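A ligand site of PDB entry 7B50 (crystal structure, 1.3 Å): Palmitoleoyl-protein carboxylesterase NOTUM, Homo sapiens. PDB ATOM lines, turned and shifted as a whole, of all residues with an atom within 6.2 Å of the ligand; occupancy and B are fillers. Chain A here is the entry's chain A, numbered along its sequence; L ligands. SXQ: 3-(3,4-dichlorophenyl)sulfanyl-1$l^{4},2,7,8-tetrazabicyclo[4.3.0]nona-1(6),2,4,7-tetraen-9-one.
The side-chain hydroxyl (OH) of Tyr 105 sits at hydrogen-bond distance from the backbone carbonyl oxygen (O) of Trp 51 (2.6 Å). N of Val 110 lies within hydrogen-bond range of OH of Tyr 105, at 2.8 Å. O of Ser 154 sits close to N of Gly 49 (3.4 Å). The side-chain hydroxyl of Thr 159 is in hydrogen-bond range of the backbone carbonyl oxygen of Gly 189, at 2.9 Å. The backbone NH (N) of Ala 265 sits at hydrogen-bond distance from the side-chain carboxylate (OD2) of Asp 263.
Gly 49 touches the ligand (C to O14, 3.95 Å). Tyr 52 touches the ligand (CD1 to S09, 3.6 Å). CG2 of Val 110 touches S09 of the ligand, at 3.7 Å. Ser 155 touches the ligand (CB to O14, 3.3 Å). Thr 159 touches the ligand (OG1 to C04, 3.2 Å). Phe 191 touches the ligand (CD2 to C03, 3.4 Å). Pro 210 touches the ligand (O to CL2, 3.8 Å). CG1 of Ile 214 touches CL2 of the ligand, at 3.3 Å. Phe 242 touches the ligand (O to CL1, 3.0 Å). Phe 243 touches the ligand (CE1 to CL1, 3.0 Å). CB of Ala 265 touches N16 of the ligand (3.3 Å). Hydrophobic or aromatic side chains that line the ligand: Trp 51, Tyr 52, Val 110, Ala 156, Phe 191, Ile 214, Phe 242, Phe 243 and Ala 265. The nearest printed residue that does not touch the ligand is Thr 211 (4.6 Å).
The backbone NH (N) of Gly 50 lies within hydrogen-bond range of an oxygen (O14) of the ligand (2.9 Å). The backbone NH of Trp 51 is in hydrogen-bond range of an oxygen (O14) of the ligand, 2.7 Å away. The backbone NH (N) of Ala 156 is in hydrogen-bond range of an oxygen (O14) of the ligand (3.2 Å).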
ATOM      1  N   GLY A  49     -12.943 -13.375   2.134  1.00  0.00           N
ATOM      2  CA  GLY A  49     -11.503 -13.282   2.073  1.00  0.00           C
ATOM      3  C   GLY A  49     -10.816 -14.602   2.404  1.00  0.00           C
ATOM      4  O   GLY A  49     -11.428 -15.674   2.471  1.00  0.00           O
ATOM      5  N   GLY A  50      -9.492 -14.520   2.597  1.00  0.00           N
ATOM      6  CA  GLY A  50      -8.694 -15.700   2.881  1.00  0.00           C
ATOM      7  C   GLY A  50      -7.359 -15.754   2.147  1.00  0.00           C
ATOM      8  O   GLY A  50      -7.005 -16.788   1.591  1.00  0.00           O
ATOM      9  N   TRP A  51      -6.607 -14.661   2.162  1.00  0.00           N
ATOM     10  CA  TRP A  51      -5.240 -14.611   1.580  1.00  0.00           C
ATOM     11  C   TRP A  51      -5.303 -14.999   0.093  1.00  0.00           C
ATOM     12  O   TRP A  51      -6.212 -14.549  -0.621  1.00  0.00           O
ATOM     13  CB  TRP A  51      -4.235 -15.351   2.424  1.00  0.00           C
ATOM     14  CG  TRP A  51      -4.051 -14.717   3.748  1.00  0.00           C
ATOM     15  CD1 TRP A  51      -4.693 -15.033   4.905  1.00  0.00           C
ATOM     16  CD2 TRP A  51      -3.181 -13.618   4.059  1.00  0.00           C
ATOM     17  NE1 TRP A  51      -4.264 -14.210   5.920  1.00  0.00           N
ATOM     18  CE2 TRP A  51      -3.338 -13.335   5.419  1.00  0.00           C
ATOM     19  CE3 TRP A  51      -2.289 -12.862   3.302  1.00  0.00           C
ATOM     20  CZ2 TRP A  51      -2.624 -12.316   6.064  1.00  0.00           C
ATOM     21  CZ3 TRP A  51      -1.564 -11.862   3.943  1.00  0.00           C
ATOM     22  CH2 TRP A  51      -1.747 -11.594   5.307  1.00  0.00           C
ATOM     23  N   TYR A  52      -4.352 -15.801  -0.389  1.00  0.00           N
ATOM     24  CA  TYR A  52      -4.190 -16.130  -1.806  1.00  0.00           C
ATOM     25  C   TYR A  52      -3.043 -17.132  -1.893  1.00  0.00           C
ATOM     26  O   TYR A  52      -2.402 -17.443  -0.895  1.00  0.00           O
ATOM     27  CB  TYR A  52      -3.904 -14.875  -2.647  1.00  0.00           C
ATOM     28  CG  TYR A  52      -2.662 -14.129  -2.217  1.00  0.00           C
ATOM     29  CD1 TYR A  52      -2.749 -13.104  -1.284  1.00  0.00           C
ATOM     30  CD2 TYR A  52      -1.422 -14.426  -2.762  1.00  0.00           C
ATOM     31  CE1 TYR A  52      -1.611 -12.407  -0.882  1.00  0.00           C
ATOM     32  CE2 TYR A  52      -0.281 -13.728  -2.382  1.00  0.00           C
ATOM     33  CZ  TYR A  52      -0.381 -12.718  -1.438  1.00  0.00           C
ATOM     34  OH  TYR A  52       0.739 -12.028  -1.049  1.00  0.00           O
ATOM     35  N   TYR A 105     -14.978 -17.445  -1.558  1.00  0.00           N
ATOM     36  CA  TYR A 105     -13.687 -17.195  -2.182  1.00  0.00           C
ATOM     37  C   TYR A 105     -13.037 -18.543  -2.456  1.00  0.00           C
ATOM     38  O   TYR A 105     -12.608 -19.239  -1.531  1.00  0.00           O
ATOM     39  CB  TYR A 105     -12.864 -16.363  -1.204  1.00  0.00           C
ATOM     40  CG  TYR A 105     -11.480 -15.978  -1.643  1.00  0.00           C
ATOM     41  CD1 TYR A 105     -11.216 -15.536  -2.932  1.00  0.00           C
ATOM     42  CD2 TYR A 105     -10.438 -15.950  -0.718  1.00  0.00           C
ATOM     43  CE1 TYR A 105      -9.946 -15.125  -3.319  1.00  0.00           C
ATOM     44  CE2 TYR A 105      -9.168 -15.551  -1.074  1.00  0.00           C
ATOM     45  CZ  TYR A 105      -8.928 -15.138  -2.378  1.00  0.00           C
ATOM     46  OH  TYR A 105      -7.665 -14.730  -2.720  1.00  0.00           O
ATOM     47  N   VAL A 110      -7.175 -13.020  -4.936  1.00  0.00           N
ATOM     48  CA  VAL A 110      -7.634 -11.729  -4.445  1.00  0.00           C
ATOM     49  C   VAL A 110      -8.731 -11.221  -5.399  1.00  0.00           C
ATOM     50  O   VAL A 110      -8.891 -10.009  -5.622  1.00  0.00           O
ATOM     51  CB  VAL A 110      -6.475 -10.729  -4.290  1.00  0.00           C
ATOM     52  CG1 VAL A 110      -6.914  -9.502  -3.514  1.00  0.00           C
ATOM     53  CG2 VAL A 110      -5.246 -11.367  -3.637  1.00  0.00           C
ATOM     54  N   SER A 154     -14.508  -8.606   2.767  1.00  0.00           N
ATOM     55  CA  SER A 154     -13.563  -8.497   3.877  1.00  0.00           C
ATOM     56  C   SER A 154     -12.224  -9.118   3.533  1.00  0.00           C
ATOM     57  O   SER A 154     -12.159 -10.192   2.907  1.00  0.00           O
ATOM     58  CB  SER A 154     -14.096  -9.133   5.168  1.00  0.00           C
ATOM     59  OG  SER A 154     -15.276  -8.496   5.637  1.00  0.00           O
ATOM     60  N   SER A 155     -11.153  -8.437   3.942  1.00  0.00           N
ATOM     61  CA  SER A 155      -9.770  -8.933   3.802  1.00  0.00           C
ATOM     62  C   SER A 155      -9.433  -9.049   2.321  1.00  0.00           C
ATOM     63  O   SER A 155      -9.519  -8.031   1.603  1.00  0.00           O
ATOM     64  CB  SER A 155      -9.554 -10.184   4.658  1.00  0.00           C
ATOM     65  OG  SER A 155      -9.891  -9.928   6.012  1.00  0.00           O
ATOM     66  N   ALA A 156      -9.012 -10.217   1.808  1.00  0.00           N
ATOM     67  CA  ALA A 156      -8.830 -10.341   0.365  1.00  0.00           C
ATOM     68  C   ALA A 156     -10.097  -9.962  -0.395  1.00  0.00           C
ATOM     69  O   ALA A 156     -10.018  -9.451  -1.514  1.00  0.00           O
ATOM     70  CB  ALA A 156      -8.380 -11.765   0.001  1.00  0.00           C
ATOM     71  N   GLY A 157     -11.271 -10.186   0.203  1.00  0.00           N
ATOM     72  CA  GLY A 157     -12.502  -9.746  -0.412  1.00  0.00           C
ATOM     73  C   GLY A 157     -12.687  -8.240  -0.410  1.00  0.00           C
ATOM     74  O   GLY A 157     -13.334  -7.688  -1.296  1.00  0.00           O
ATOM     75  N   THR A 159     -10.092  -6.035  -0.703  1.00  0.00           N
ATOM     76  CA  THR A 159      -9.301  -5.652  -1.873  1.00  0.00           C
ATOM     77  C   THR A 159     -10.025  -6.035  -3.158  1.00  0.00           C
ATOM     78  O   THR A 159     -10.029  -5.261  -4.122  1.00  0.00           O
ATOM     79  CB  THR A 159      -7.914  -6.305  -1.817  1.00  0.00           C
ATOM     80  OG1 THR A 159      -7.340  -6.083  -0.514  1.00  0.00           O
ATOM     81  CG2 THR A 159      -6.999  -5.749  -2.890  1.00  0.00           C
ATOM     82  N   SER A 188     -11.227  -4.072   5.609  1.00  0.00           N
ATOM     83  CA  SER A 188      -9.965  -4.728   5.954  1.00  0.00           C
ATOM     84  C   SER A 188      -9.176  -5.133   4.712  1.00  0.00           C
ATOM     85  O   SER A 188      -8.422  -6.118   4.738  1.00  0.00           O
ATOM     86  CB  SER A 188     -10.207  -5.903   6.893  1.00  0.00           C
ATOM     87  OG  SER A 188     -10.845  -5.450   8.088  1.00  0.00           O
ATOM     88  N   GLY A 189      -9.298  -4.358   3.640  1.00  0.00           N
ATOM     89  CA  GLY A 189      -8.581  -4.630   2.412  1.00  0.00           C
ATOM     90  C   GLY A 189      -7.729  -3.466   1.940  1.00  0.00           C
ATOM     91  O   GLY A 189      -7.317  -3.438   0.772  1.00  0.00           O
ATOM     92  N   PHE A 191      -4.326  -1.772   2.451  1.00  0.00           N
ATOM     93  CA  PHE A 191      -3.010  -2.075   2.992  1.00  0.00           C
ATOM     94  C   PHE A 191      -1.983  -1.059   2.538  1.00  0.00           C
ATOM     95  O   PHE A 191      -2.164  -0.360   1.534  1.00  0.00           O
ATOM     96  CB  PHE A 191      -2.582  -3.487   2.562  1.00  0.00           C
ATOM     97  CG  PHE A 191      -3.495  -4.532   3.073  1.00  0.00           C
ATOM     98  CD1 PHE A 191      -3.556  -4.773   4.427  1.00  0.00           C
ATOM     99  CD2 PHE A 191      -4.355  -5.205   2.225  1.00  0.00           C
ATOM    100  CE1 PHE A 191      -4.447  -5.716   4.925  1.00  0.00           C
ATOM    101  CE2 PHE A 191      -5.230  -6.145   2.721  1.00  0.00           C
ATOM    102  CZ  PHE A 191      -5.276  -6.402   4.064  1.00  0.00           C
ATOM    103  N   LEU A 192      -0.872  -1.004   3.267  1.00  0.00           N
ATOM    104  CA  LEU A 192       0.247  -0.144   2.932  1.00  0.00           C
ATOM    105  C   LEU A 192       1.415  -0.996   2.476  1.00  0.00           C
ATOM    106  O   LEU A 192       1.738  -2.009   3.122  1.00  0.00           O
ATOM    107  CB  LEU A 192       0.674   0.658   4.168  1.00  0.00           C
ATOM    108  CG  LEU A 192      -0.395   1.527   4.816  1.00  0.00           C
ATOM    109  CD1 LEU A 192       0.206   2.292   5.978  1.00  0.00           C
ATOM    110  CD2 LEU A 192      -0.976   2.512   3.794  1.00  0.00           C
ATOM    111  N   PRO A 210       5.621  -9.380   0.431  1.00  0.00           N
ATOM    112  CA  PRO A 210       4.202  -9.397   0.051  1.00  0.00           C
ATOM    113  C   PRO A 210       3.951  -8.765  -1.326  1.00  0.00           C
ATOM    114  O   PRO A 210       3.127  -9.275  -2.077  1.00  0.00           O
ATOM    115  CB  PRO A 210       3.536  -8.552   1.151  1.00  0.00           C
ATOM    116  CG  PRO A 210       4.447  -8.694   2.318  1.00  0.00           C
ATOM    117  CD  PRO A 210       5.832  -8.761   1.750  1.00  0.00           C
ATOM    118  N   THR A 211       4.654  -7.678  -1.631  1.00  0.00           N
ATOM    119  CA  THR A 211       4.508  -7.088  -2.963  1.00  0.00           C
ATOM    120  C   THR A 211       5.108  -7.991  -4.026  1.00  0.00           C
ATOM    121  O   THR A 211       4.592  -8.060  -5.153  1.00  0.00           O
ATOM    122  CB  THR A 211       5.171  -5.705  -3.013  1.00  0.00           C
ATOM    123  OG1 THR A 211       6.575  -5.847  -2.753  1.00  0.00           O
ATOM    124  CG2 THR A 211       4.544  -4.778  -1.988  1.00  0.00           C
ATOM    125  N   ILE A 214       2.419 -10.732  -4.635  1.00  0.00           N
ATOM    126  CA  ILE A 214       1.362 -10.229  -5.510  1.00  0.00           C
ATOM    127  C   ILE A 214       1.848 -10.101  -6.946  1.00  0.00           C
ATOM    128  O   ILE A 214       1.149 -10.473  -7.896  1.00  0.00           O
ATOM    129  CB  ILE A 214       0.766  -8.922  -4.971  1.00  0.00           C
ATOM    130  CG1 ILE A 214      -0.005  -9.187  -3.674  1.00  0.00           C
ATOM    131  CG2 ILE A 214      -0.139  -8.261  -6.022  1.00  0.00           C
ATOM    132  CD1 ILE A 214      -1.111 -10.235  -3.837  1.00  0.00           C
ATOM    133  N   TRP A 239       0.655  -4.499  -9.825  1.00  0.00           N
ATOM    134  CA  TRP A 239       0.589  -4.784  -8.396  1.00  0.00           C
ATOM    135  C   TRP A 239       0.227  -3.540  -7.584  1.00  0.00           C
ATOM    136  O   TRP A 239      -0.370  -3.659  -6.519  1.00  0.00           O
ATOM    137  CB  TRP A 239       1.933  -5.356  -7.920  1.00  0.00           C
ATOM    138  CG  TRP A 239       3.080  -4.352  -7.989  1.00  0.00           C
ATOM    139  CD1 TRP A 239       3.958  -4.190  -9.013  1.00  0.00           C
ATOM    140  CD2 TRP A 239       3.418  -3.375  -6.984  1.00  0.00           C
ATOM    141  NE1 TRP A 239       4.840  -3.171  -8.710  1.00  0.00           N
ATOM    142  CE2 TRP A 239       4.525  -2.657  -7.479  1.00  0.00           C
ATOM    143  CE3 TRP A 239       2.889  -3.033  -5.737  1.00  0.00           C
ATOM    144  CZ2 TRP A 239       5.127  -1.604  -6.741  1.00  0.00           C
ATOM    145  CZ3 TRP A 239       3.485  -1.989  -5.019  1.00  0.00           C
ATOM    146  CH2 TRP A 239       4.585  -1.298  -5.529  1.00  0.00           C
ATOM    147  N   PHE A 242      -3.351  -3.127  -6.277  1.00  0.00           N
ATOM    148  CA  PHE A 242      -3.832  -3.894  -5.144  1.00  0.00           C
ATOM    149  C   PHE A 242      -3.769  -3.096  -3.851  1.00  0.00           C
ATOM    150  O   PHE A 242      -4.286  -3.561  -2.825  1.00  0.00           O
ATOM    151  CB  PHE A 242      -3.006  -5.197  -4.989  1.00  0.00           C
ATOM    152  CG  PHE A 242      -3.414  -6.280  -5.934  1.00  0.00           C
ATOM    153  CD1 PHE A 242      -3.295  -6.113  -7.307  1.00  0.00           C
ATOM    154  CD2 PHE A 242      -3.869  -7.501  -5.444  1.00  0.00           C
ATOM    155  CE1 PHE A 242      -3.685  -7.135  -8.178  1.00  0.00           C
ATOM    156  CE2 PHE A 242      -4.247  -8.523  -6.308  1.00  0.00           C
ATOM    157  CZ  PHE A 242      -4.150  -8.334  -7.669  1.00  0.00           C
ATOM    158  N   PHE A 243      -3.161  -1.913  -3.867  1.00  0.00           N
ATOM    159  CA  PHE A 243      -3.042  -1.094  -2.683  1.00  0.00           C
ATOM    160  C   PHE A 243      -4.097   0.001  -2.712  1.00  0.00           C
ATOM    161  O   PHE A 243      -4.110   0.832  -3.628  1.00  0.00           O
ATOM    162  CB  PHE A 243      -1.618  -0.560  -2.554  1.00  0.00           C
ATOM    163  CG  PHE A 243      -0.643  -1.645  -2.182  1.00  0.00           C
ATOM    164  CD1 PHE A 243      -0.416  -1.951  -0.845  1.00  0.00           C
ATOM    165  CD2 PHE A 243      -0.088  -2.447  -3.148  1.00  0.00           C
ATOM    166  CE1 PHE A 243       0.453  -2.976  -0.487  1.00  0.00           C
ATOM    167  CE2 PHE A 243       0.758  -3.485  -2.807  1.00  0.00           C
ATOM    168  CZ  PHE A 243       1.023  -3.747  -1.466  1.00  0.00           C
ATOM    169  N   GLY A 244      -4.998  -0.053  -1.722  1.00  0.00           N
ATOM    170  CA  GLY A 244      -6.176   0.825  -1.711  1.00  0.00           C
ATOM    171  C   GLY A 244      -5.863   2.277  -1.993  1.00  0.00           C
ATOM    172  O   GLY A 244      -6.536   2.915  -2.814  1.00  0.00           O
ATOM    173  N   ASP A 263      -4.331  -2.906  11.647  1.00  0.00           N
ATOM    174  CA  ASP A 263      -4.882  -4.176  11.186  1.00  0.00           C
ATOM    175  C   ASP A 263      -3.892  -5.304  11.435  1.00  0.00           C
ATOM    176  O   ASP A 263      -2.694  -5.166  11.162  1.00  0.00           O
ATOM    177  CB  ASP A 263      -5.210  -4.039   9.692  1.00  0.00           C
ATOM    178  CG  ASP A 263      -5.840  -5.273   9.135  1.00  0.00           C
ATOM    179  OD1 ASP A 263      -7.089  -5.366   9.135  1.00  0.00           O
ATOM    180  OD2 ASP A 263      -5.073  -6.161   8.701  1.00  0.00           O
ATOM    181  N   ALA A 265      -3.448  -8.147   9.988  1.00  0.00           N
ATOM    182  CA  ALA A 265      -2.777  -8.700   8.810  1.00  0.00           C
ATOM    183  C   ALA A 265      -1.693  -7.763   8.310  1.00  0.00           C
ATOM    184  O   ALA A 265      -0.634  -8.217   7.842  1.00  0.00           O
ATOM    185  CB  ALA A 265      -3.787  -9.009   7.706  1.00  0.00           C
ATOM    186  N   GLN A 266      -1.926  -6.443   8.394  1.00  0.00           N
ATOM    187  CA  GLN A 266      -0.885  -5.468   8.099  1.00  0.00           C
ATOM    188  C   GLN A 266       0.322  -5.683   9.004  1.00  0.00           C
ATOM    189  O   GLN A 266       1.465  -5.741   8.548  1.00  0.00           O
ATOM    190  CB  GLN A 266      -1.429  -4.054   8.275  1.00  0.00           C
ATOM    191  CG  GLN A 266      -0.392  -2.959   7.986  1.00  0.00           C
ATOM    192  CD  GLN A 266      -0.123  -2.767   6.507  1.00  0.00           C
ATOM    193  OE1 GLN A 266      -1.067  -2.601   5.712  1.00  0.00           O
ATOM    194  NE2 GLN A 266       1.146  -2.779   6.100  1.00  0.00           N
ATOM    195  N   VAL A 269       2.290  -9.012   8.007  1.00  0.00           N
ATOM    196  CA  VAL A 269       3.203  -8.838   6.885  1.00  0.00           C
ATOM    197  C   VAL A 269       4.350  -7.902   7.247  1.00  0.00           C
ATOM    198  O   VAL A 269       5.443  -8.017   6.690  1.00  0.00           O
ATOM    199  CB  VAL A 269       2.455  -8.410   5.596  1.00  0.00           C
ATOM    200  CG1 VAL A 269       1.381  -9.430   5.231  1.00  0.00           C
ATOM    201  CG2 VAL A 269       1.874  -7.015   5.720  1.00  0.00           C
HETATM  202  C02 SXQ L   1      -2.519  -6.292  -1.027  1.00  0.00           C
HETATM  203  C03 SXQ L   1      -3.877  -6.363  -0.939  1.00  0.00           C
HETATM  204  C04 SXQ L   1      -4.487  -7.564  -0.689  1.00  0.00           C
HETATM  205  C05 SXQ L   1      -3.687  -8.667  -0.550  1.00  0.00           C
HETATM  206  C06 SXQ L   1      -2.302  -8.625  -0.627  1.00  0.00           C
HETATM  207  C07 SXQ L   1      -1.703  -7.405  -0.873  1.00  0.00           C
HETATM  208  C10 SXQ L   1      -4.684 -10.230   1.551  1.00  0.00           C
HETATM  209  C13 SXQ L   1      -6.798 -11.900   4.029  1.00  0.00           C
HETATM  210  C17 SXQ L   1      -5.057 -10.435   4.264  1.00  0.00           C
HETATM  211  C18 SXQ L   1      -4.040  -9.602   3.803  1.00  0.00           C
HETATM  212  C19 SXQ L   1      -3.836  -9.489   2.436  1.00  0.00           C
HETATM  213  N11 SXQ L   1      -5.635 -11.017   2.007  1.00  0.00           N
HETATM  214  N12 SXQ L   1      -5.812 -11.101   3.352  1.00  0.00           N
HETATM  215  N15 SXQ L   1      -6.638 -11.705   5.425  1.00  0.00           N
HETATM  216  N16 SXQ L   1      -5.579 -10.803   5.604  1.00  0.00           N
HETATM  217  O14 SXQ L   1      -7.609 -12.557   3.471  1.00  0.00           O
HETATM  218  S09 SXQ L   1      -4.548 -10.202  -0.222  1.00  0.00           S
HETATM  219 CL1  SXQ L   1      -1.931  -4.660  -1.351  1.00  0.00          CL
HETATM  220 CL2  SXQ L   1       0.082  -7.329  -0.985  1.00  0.00          CL
